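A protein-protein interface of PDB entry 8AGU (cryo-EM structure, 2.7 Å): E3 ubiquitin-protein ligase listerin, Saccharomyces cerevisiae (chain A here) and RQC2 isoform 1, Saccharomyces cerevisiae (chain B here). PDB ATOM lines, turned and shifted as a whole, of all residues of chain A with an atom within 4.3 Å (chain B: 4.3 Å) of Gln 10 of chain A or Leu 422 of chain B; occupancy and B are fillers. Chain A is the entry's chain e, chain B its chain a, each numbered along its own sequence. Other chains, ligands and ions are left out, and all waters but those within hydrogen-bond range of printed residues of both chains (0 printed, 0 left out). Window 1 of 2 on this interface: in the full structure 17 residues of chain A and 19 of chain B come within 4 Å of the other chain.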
ATOM      1  N   ASN A   7      -2.744  10.367 -16.130  1.00  0.00           N
ATOM      2  CA  ASN A   7      -3.328  10.353 -17.469  1.00  0.00           C
ATOM      3  C   ASN A   7      -4.841  10.283 -17.378  1.00  0.00           C
ATOM      4  O   ASN A   7      -5.429   9.243 -17.662  1.00  0.00           O
ATOM      5  CB  ASN A   7      -2.823   9.148 -18.263  1.00  0.00           C
ATOM      6  CG  ASN A   7      -1.319   9.153 -18.456  1.00  0.00           C
ATOM      7  OD1 ASN A   7      -0.604   9.953 -17.859  1.00  0.00           O
ATOM      8  ND2 ASN A   7      -0.830   8.243 -19.290  1.00  0.00           N
ATOM      9  N   THR A   8      -5.479  11.387 -17.005  1.00  0.00           N
ATOM     10  CA  THR A   8      -6.928  11.389 -16.822  1.00  0.00           C
ATOM     11  C   THR A   8      -7.699  11.085 -18.095  1.00  0.00           C
ATOM     12  O   THR A   8      -8.649  10.312 -18.070  1.00  0.00           O
ATOM     13  CB  THR A   8      -7.407  12.751 -16.298  1.00  0.00           C
ATOM     14  OG1 THR A   8      -7.042  13.773 -17.232  1.00  0.00           O
ATOM     15  CG2 THR A   8      -6.774  13.056 -14.954  1.00  0.00           C
ATOM     16  N   PHE A   9      -7.287  11.676 -19.208  1.00  0.00           N
ATOM     17  CA  PHE A   9      -7.997  11.469 -20.463  1.00  0.00           C
ATOM     18  C   PHE A   9      -7.944  10.020 -20.903  1.00  0.00           C
ATOM     19  O   PHE A   9      -8.936   9.480 -21.387  1.00  0.00           O
ATOM     20  CB  PHE A   9      -7.460  12.389 -21.555  1.00  0.00           C
ATOM     21  CG  PHE A   9      -8.038  13.771 -21.511  1.00  0.00           C
ATOM     22  CD1 PHE A   9      -9.295  14.020 -22.026  1.00  0.00           C
ATOM     23  CD2 PHE A   9      -7.332  14.816 -20.948  1.00  0.00           C
ATOM     24  CE1 PHE A   9      -9.836  15.287 -21.983  1.00  0.00           C
ATOM     25  CE2 PHE A   9      -7.865  16.088 -20.904  1.00  0.00           C
ATOM     26  CZ  PHE A   9      -9.122  16.324 -21.420  1.00  0.00           C
ATOM     27  N   GLN A  10      -6.788   9.387 -20.740  1.00  0.00           N
ATOM     28  CA  GLN A  10      -6.660   7.978 -21.087  1.00  0.00           C
ATOM     29  C   GLN A  10      -7.571   7.143 -20.208  1.00  0.00           C
ATOM     30  O   GLN A  10      -8.194   6.188 -20.674  1.00  0.00           O
ATOM     31  CB  GLN A  10      -5.211   7.519 -20.930  1.00  0.00           C
ATOM     32  CG  GLN A  10      -4.194   8.400 -21.638  1.00  0.00           C
ATOM     33  CD  GLN A  10      -4.184   8.219 -23.145  1.00  0.00           C
ATOM     34  OE1 GLN A  10      -4.803   7.300 -23.683  1.00  0.00           O
ATOM     35  NE2 GLN A  10      -3.464   9.094 -23.834  1.00  0.00           N
ATOM     36  N   GLN A  11      -7.647   7.495 -18.930  1.00  0.00           N
ATOM     37  CA  GLN A  11      -8.507   6.766 -18.006  1.00  0.00           C
ATOM     38  C   GLN A  11      -9.969   6.872 -18.398  1.00  0.00           C
ATOM     39  O   GLN A  11     -10.705   5.901 -18.293  1.00  0.00           O
ATOM     40  CB  GLN A  11      -8.304   7.268 -16.580  1.00  0.00           C
ATOM     41  CG  GLN A  11      -6.969   6.863 -15.984  1.00  0.00           C
ATOM     42  CD  GLN A  11      -6.608   7.677 -14.761  1.00  0.00           C
ATOM     43  OE1 GLN A  11      -7.262   8.671 -14.447  1.00  0.00           O
ATOM     44  NE2 GLN A  11      -5.555   7.264 -14.067  1.00  0.00           N
ATOM     45  N   TYR A  12     -10.400   8.050 -18.834  1.00  0.00           N
ATOM     46  CA  TYR A  12     -11.776   8.202 -19.297  1.00  0.00           C
ATOM     47  C   TYR A  12     -12.011   7.343 -20.526  1.00  0.00           C
ATOM     48  O   TYR A  12     -13.071   6.737 -20.669  1.00  0.00           O
ATOM     49  CB  TYR A  12     -12.095   9.657 -19.641  1.00  0.00           C
ATOM     50  CG  TYR A  12     -11.794  10.669 -18.558  1.00  0.00           C
ATOM     51  CD1 TYR A  12     -11.995  10.371 -17.218  1.00  0.00           C
ATOM     52  CD2 TYR A  12     -11.330  11.936 -18.885  1.00  0.00           C
ATOM     53  CE1 TYR A  12     -11.722  11.299 -16.232  1.00  0.00           C
ATOM     54  CE2 TYR A  12     -11.054  12.872 -17.908  1.00  0.00           C
ATOM     55  CZ  TYR A  12     -11.253  12.549 -16.583  1.00  0.00           C
ATOM     56  OH  TYR A  12     -10.983  13.479 -15.607  1.00  0.00           O
ATOM     57  N   ASN A  13     -11.027   7.289 -21.420  1.00  0.00           N
ATOM     58  CA  ASN A  13     -11.183   6.541 -22.667  1.00  0.00           C
ATOM     59  C   ASN A  13     -11.405   5.049 -22.451  1.00  0.00           C
ATOM     60  O   ASN A  13     -12.202   4.444 -23.166  1.00  0.00           O
ATOM     61  CB  ASN A  13      -9.956   6.756 -23.557  1.00  0.00           C
ATOM     62  CG  ASN A  13     -10.223   6.433 -25.014  1.00  0.00           C
ATOM     63  OD1 ASN A  13     -11.370   6.427 -25.464  1.00  0.00           O
ATOM     64  ND2 ASN A  13      -9.160   6.178 -25.765  1.00  0.00           N
ATOM     65  N   THR A  14     -10.688   4.452 -21.501  1.00  0.00           N
ATOM     66  CA  THR A  14     -10.822   3.013 -21.206  1.00  0.00           C
ATOM     67  C   THR A  14     -10.627   2.105 -22.419  1.00  0.00           C
ATOM     68  O   THR A  14     -11.359   1.129 -22.583  1.00  0.00           O
ATOM     69  CB  THR A  14     -12.156   2.625 -20.510  1.00  0.00           C
ATOM     70  OG1 THR A  14     -13.245   2.694 -21.441  1.00  0.00           O
ATOM     71  CG2 THR A  14     -12.446   3.512 -19.316  1.00  0.00           C
ATOM     72  N   ARG A  24      -2.834   0.456 -21.846  1.00  0.00           N
ATOM     73  CA  ARG A  24      -3.062   0.782 -23.241  1.00  0.00           C
ATOM     74  C   ARG A  24      -1.759   0.764 -23.993  1.00  0.00           C
ATOM     75  O   ARG A  24      -0.789   1.386 -23.571  1.00  0.00           O
ATOM     76  CB  ARG A  24      -3.689   2.163 -23.394  1.00  0.00           C
ATOM     77  CG  ARG A  24      -3.806   2.596 -24.847  1.00  0.00           C
ATOM     78  CD  ARG A  24      -4.090   4.083 -24.990  1.00  0.00           C
ATOM     79  NE  ARG A  24      -4.169   4.473 -26.395  1.00  0.00           N
ATOM     80  CZ  ARG A  24      -5.298   4.533 -27.093  1.00  0.00           C
ATOM     81  NH1 ARG A  24      -6.455   4.241 -26.515  1.00  0.00           N
ATOM     82  NH2 ARG A  24      -5.274   4.891 -28.369  1.00  0.00           N
ATOM     83  N   PHE A  30       1.156  10.284 -29.717  1.00  0.00           N
ATOM     84  CA  PHE A  30       0.425  11.005 -28.674  1.00  0.00           C
ATOM     85  C   PHE A  30      -0.036  10.143 -27.504  1.00  0.00           C
ATOM     86  O   PHE A  30      -0.035  10.602 -26.365  1.00  0.00           O
ATOM     87  CB  PHE A  30      -0.718  11.869 -29.235  1.00  0.00           C
ATOM     88  CG  PHE A  30      -1.488  11.236 -30.357  1.00  0.00           C
ATOM     89  CD1 PHE A  30      -2.583  10.435 -30.096  1.00  0.00           C
ATOM     90  CD2 PHE A  30      -1.141  11.482 -31.674  1.00  0.00           C
ATOM     91  CE1 PHE A  30      -3.300   9.861 -31.127  1.00  0.00           C
ATOM     92  CE2 PHE A  30      -1.854  10.914 -32.709  1.00  0.00           C
ATOM     93  CZ  PHE A  30      -2.937  10.103 -32.436  1.00  0.00           C
ATOM     94  N   ASP A  31      -0.436   8.908 -27.767  1.00  0.00           N
ATOM     95  CA  ASP A  31      -0.975   8.066 -26.700  1.00  0.00           C
ATOM     96  C   ASP A  31      -0.219   6.767 -26.479  1.00  0.00           C
ATOM     97  O   ASP A  31       0.536   6.332 -27.340  1.00  0.00           O
ATOM     98  CB  ASP A  31      -2.466   7.787 -26.922  1.00  0.00           C
ATOM     99  CG  ASP A  31      -2.789   7.385 -28.350  1.00  0.00           C
ATOM    100  OD1 ASP A  31      -1.867   7.030 -29.110  1.00  0.00           O
ATOM    101  OD2 ASP A  31      -3.981   7.426 -28.716  1.00  0.00           O
ATOM    102  N   LEU B 409      -2.060  16.549 -17.782  1.00  0.00           N
ATOM    103  CA  LEU B 409      -1.193  16.496 -18.950  1.00  0.00           C
ATOM    104  C   LEU B 409      -0.042  17.481 -18.830  1.00  0.00           C
ATOM    105  O   LEU B 409       1.094  17.157 -19.167  1.00  0.00           O
ATOM    106  CB  LEU B 409      -1.988  16.778 -20.223  1.00  0.00           C
ATOM    107  CG  LEU B 409      -2.689  15.613 -20.926  1.00  0.00           C
ATOM    108  CD1 LEU B 409      -1.686  14.533 -21.288  1.00  0.00           C
ATOM    109  CD2 LEU B 409      -3.819  15.027 -20.098  1.00  0.00           C
ATOM    110  N   THR B 418       1.752  18.218 -28.736  1.00  0.00           N
ATOM    111  CA  THR B 418       1.347  16.825 -28.621  1.00  0.00           C
ATOM    112  C   THR B 418       0.085  16.710 -27.785  1.00  0.00           C
ATOM    113  O   THR B 418      -0.780  15.885 -28.069  1.00  0.00           O
ATOM    114  CB  THR B 418       2.448  15.926 -28.040  1.00  0.00           C
ATOM    115  OG1 THR B 418       2.538  16.118 -26.624  1.00  0.00           O
ATOM    116  CG2 THR B 418       3.787  16.235 -28.689  1.00  0.00           C
ATOM    117  N   ILE B 419      -0.024  17.533 -26.750  1.00  0.00           N
ATOM    118  CA  ILE B 419      -1.191  17.473 -25.893  1.00  0.00           C
ATOM    119  C   ILE B 419      -2.410  17.779 -26.738  1.00  0.00           C
ATOM    120  O   ILE B 419      -3.419  17.082 -26.659  1.00  0.00           O
ATOM    121  CB  ILE B 419      -1.114  18.503 -24.750  1.00  0.00           C
ATOM    122  CG1 ILE B 419      -0.032  18.118 -23.746  1.00  0.00           C
ATOM    123  CG2 ILE B 419      -2.445  18.619 -24.022  1.00  0.00           C
ATOM    124  CD1 ILE B 419       0.146  19.123 -22.630  1.00  0.00           C
ATOM    125  N   GLU B 420      -2.301  18.785 -27.595  1.00  0.00           N
ATOM    126  CA  GLU B 420      -3.437  19.160 -28.422  1.00  0.00           C
ATOM    127  C   GLU B 420      -3.845  18.039 -29.369  1.00  0.00           C
ATOM    128  O   GLU B 420      -5.029  17.779 -29.543  1.00  0.00           O
ATOM    129  CB  GLU B 420      -3.160  20.451 -29.187  1.00  0.00           C
ATOM    130  CG  GLU B 420      -3.081  21.676 -28.293  1.00  0.00           C
ATOM    131  CD  GLU B 420      -3.265  22.971 -29.057  1.00  0.00           C
ATOM    132  OE1 GLU B 420      -3.606  22.912 -30.257  1.00  0.00           O
ATOM    133  OE2 GLU B 420      -3.075  24.049 -28.457  1.00  0.00           O
ATOM    134  N   LYS B 421      -2.872  17.360 -29.962  1.00  0.00           N
ATOM    135  CA  LYS B 421      -3.183  16.256 -30.859  1.00  0.00           C
ATOM    136  C   LYS B 421      -3.909  15.154 -30.118  1.00  0.00           C
ATOM    137  O   LYS B 421      -4.835  14.552 -30.650  1.00  0.00           O
ATOM    138  CB  LYS B 421      -1.922  15.702 -31.516  1.00  0.00           C
ATOM    139  CG  LYS B 421      -1.622  16.304 -32.877  1.00  0.00           C
ATOM    140  CD  LYS B 421      -2.668  15.894 -33.901  1.00  0.00           C
ATOM    141  CE  LYS B 421      -2.669  14.391 -34.136  1.00  0.00           C
ATOM    142  NZ  LYS B 421      -1.391  13.911 -34.731  1.00  0.00           N
ATOM    143  N   LEU B 422      -3.487  14.882 -28.894  1.00  0.00           N
ATOM    144  CA  LEU B 422      -4.142  13.858 -28.103  1.00  0.00           C
ATOM    145  C   LEU B 422      -5.590  14.240 -27.844  1.00  0.00           C
ATOM    146  O   LEU B 422      -6.474  13.393 -27.895  1.00  0.00           O
ATOM    147  CB  LEU B 422      -3.401  13.640 -26.789  1.00  0.00           C
ATOM    148  CG  LEU B 422      -3.885  12.508 -25.885  1.00  0.00           C
ATOM    149  CD1 LEU B 422      -3.971  11.200 -26.655  1.00  0.00           C
ATOM    150  CD2 LEU B 422      -2.964  12.372 -24.684  1.00  0.00           C
ATOM    151  N   ILE B 423      -5.841  15.515 -27.575  1.00  0.00           N
ATOM    152  CA  ILE B 423      -7.208  15.962 -27.342  1.00  0.00           C
ATOM    153  C   ILE B 423      -8.033  15.720 -28.598  1.00  0.00           C
ATOM    154  O   ILE B 423      -9.167  15.243 -28.527  1.00  0.00           O
ATOM    155  CB  ILE B 423      -7.269  17.454 -26.971  1.00  0.00           C
ATOM    156  CG1 ILE B 423      -6.470  17.721 -25.697  1.00  0.00           C
ATOM    157  CG2 ILE B 423      -8.706  17.913 -26.777  1.00  0.00           C
ATOM    158  CD1 ILE B 423      -6.944  16.921 -24.507  1.00  0.00           C
ATOM    159  N   LYS B 424      -7.452  16.006 -29.756  1.00  0.00           N
ATOM    160  CA  LYS B 424      -8.171  15.809 -31.002  1.00  0.00           C
ATOM    161  C   LYS B 424      -8.497  14.343 -31.136  1.00  0.00           C
ATOM    162  O   LYS B 424      -9.601  13.980 -31.534  1.00  0.00           O
ATOM    163  CB  LYS B 424      -7.311  16.238 -32.186  1.00  0.00           C
ATOM    164  CG  LYS B 424      -6.873  17.689 -32.143  1.00  0.00           C
ATOM    165  CD  LYS B 424      -5.763  17.979 -33.138  1.00  0.00           C
ATOM    166  CE  LYS B 424      -5.246  19.398 -32.970  1.00  0.00           C
ATOM    167  NZ  LYS B 424      -4.085  19.677 -33.858  1.00  0.00           N
ATOM    168  N   SER B 425      -7.540  13.494 -30.787  1.00  0.00           N
ATOM    169  CA  SER B 425      -7.746  12.060 -30.905  1.00  0.00           C
ATOM    170  C   SER B 425      -8.863  11.594 -29.997  1.00  0.00           C
ATOM    171  O   SER B 425      -9.657  10.753 -30.384  1.00  0.00           O
ATOM    172  CB  SER B 425      -6.465  11.301 -30.593  1.00  0.00           C
ATOM    173  OG  SER B 425      -6.620   9.924 -30.871  1.00  0.00           O
ATOM    174  N   GLU B 426      -8.928  12.140 -28.790  1.00  0.00           N
ATOM    175  CA  GLU B 426      -9.994  11.779 -27.866  1.00  0.00           C
ATOM    176  C   GLU B 426     -11.343  12.166 -28.441  1.00  0.00           C
ATOM    177  O   GLU B 426     -12.328  11.464 -28.238  1.00  0.00           O
ATOM    178  CB  GLU B 426      -9.786  12.413 -26.491  1.00  0.00           C
ATOM    179  CG  GLU B 426      -8.544  11.927 -25.754  1.00  0.00           C
ATOM    180  CD  GLU B 426      -8.636  10.479 -25.304  1.00  0.00           C
ATOM    181  OE1 GLU B 426      -9.760   9.978 -25.100  1.00  0.00           O
ATOM    182  OE2 GLU B 426      -7.575   9.843 -25.138  1.00  0.00           O
ATOM    183  N   LYS B 429     -12.214   9.581 -30.698  1.00  0.00           N
ATOM    184  CA  LYS B 429     -12.593   8.429 -29.886  1.00  0.00           C
ATOM    185  C   LYS B 429     -13.998   8.597 -29.344  1.00  0.00           C
ATOM    186  O   LYS B 429     -14.691   7.614 -29.094  1.00  0.00           O
ATOM    187  CB  LYS B 429     -11.598   8.217 -28.746  1.00  0.00           C
ATOM    188  CG  LYS B 429     -10.239   7.716 -29.206  1.00  0.00           C
ATOM    189  CD  LYS B 429      -9.140   8.205 -28.280  1.00  0.00           C
ATOM    190  CE  LYS B 429      -7.777   7.668 -28.678  1.00  0.00           C
ATOM    191  NZ  LYS B 429      -6.705   8.226 -27.808  1.00  0.00           N
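The side-chain amino group of Lys 429 of chain B is in salt-bridge range of the side-chain carboxylate of Asp 31 of chain A.
The side-chain carboxylate (OE2) of Glu 426 of chain B is in salt-bridge range of the side-chain amino group (NZ) of Lys 429 of chain B (3.2 Å). ND2 of Asn 13 of chain A sits close to NH1 of Arg 24 of chain A (3.4 Å). The guanidinium group (NH2) of Arg 24 of chain A is in salt-bridge range of the side-chain carboxylate (OD2) of Asp 31 of chain A, at 2.9 Å.
Leu 409 of chain B touches Phe 9 of chain A (CD2 to CD2, 3.6 Å). Ile 423 of chain B touches Phe 9 of chain A (CD1 to CE2, 3.8 Å). Glu 426 of chain B touches Phe 9 of chain A (OE1 to O, 3.8 Å). Gln 10 of chain A touches Leu 422 of chain B. CG of Asn 13 of chain A touches OE1 of Glu 426 of chain B, 3.6 Å away. Lys 429 of chain B touches Asn 13 of chain A (CD to ND2, 3.2 Å). Lys 429 of chain B touches Arg 24 of chain A. CE2 of Phe 30 of chain A touches NZ of Lys 421 of chain B, at 3.6 Å. Phe 30 of chain A touches Ser 425 of chain B. Asp 31 of chain A touches Leu 422 of chain B (CB to CD1, 3.7 Å).
Printed residues of chain B within 4 Å of Gln 10 of chain A: Leu 422 (3.4 Å). Of the printed residues of chain B, Arg 24 of chain A touches Lys 429 (3.7 Å). Of the printed residues of chain B, Asp 31 of chain A touches Leu 422 (3.7 Å) and Lys 429 (3.0 Å). Of the printed residues of chain A, Ser 425 of chain B touches Phe 30 (3.3 Å). Of the printed residues of chain A, Lys 429 of chain B touches Asn 13 (3.2 Å), Arg 24 (3.7 Å) and Asp 31 (3.0 Å). Printed residues of chain B within 4 Å of Phe 30 of chain A: Lys 421 (3.6 Å), Leu 422 (3.8 Å) and Ser 425 (3.3 Å). The nearest residue of chain B that does not touch Gln 10 of chain A is Glu 426 of chain B (4.03 Å). The nearest printed residue of chain A that does not touch Leu 422 of chain B is Phe 9 of chain A (5.5 Å). The nearest printed residue of chain A that does not touch Lys 429 of chain B is Gln 10 of chain A (4.6 Å).
Printed residues of chain A that touch a printed residue of chain B: Phe 9, Gln 10, Asn 13, Arg 24, Phe 30 and Asp 31. Printed residues of chain B that touch a printed residue of chain A: Leu 409, Lys 421, Leu 422, Ile 423, Ser 425, Glu 426 and Lys 429. Among the printed residues, Asp or Glu carboxylates within 4 Å of a Lys or Arg side-chain nitrogen of the other chain: Asp 31 of chain A with Lys 429 of chain B.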
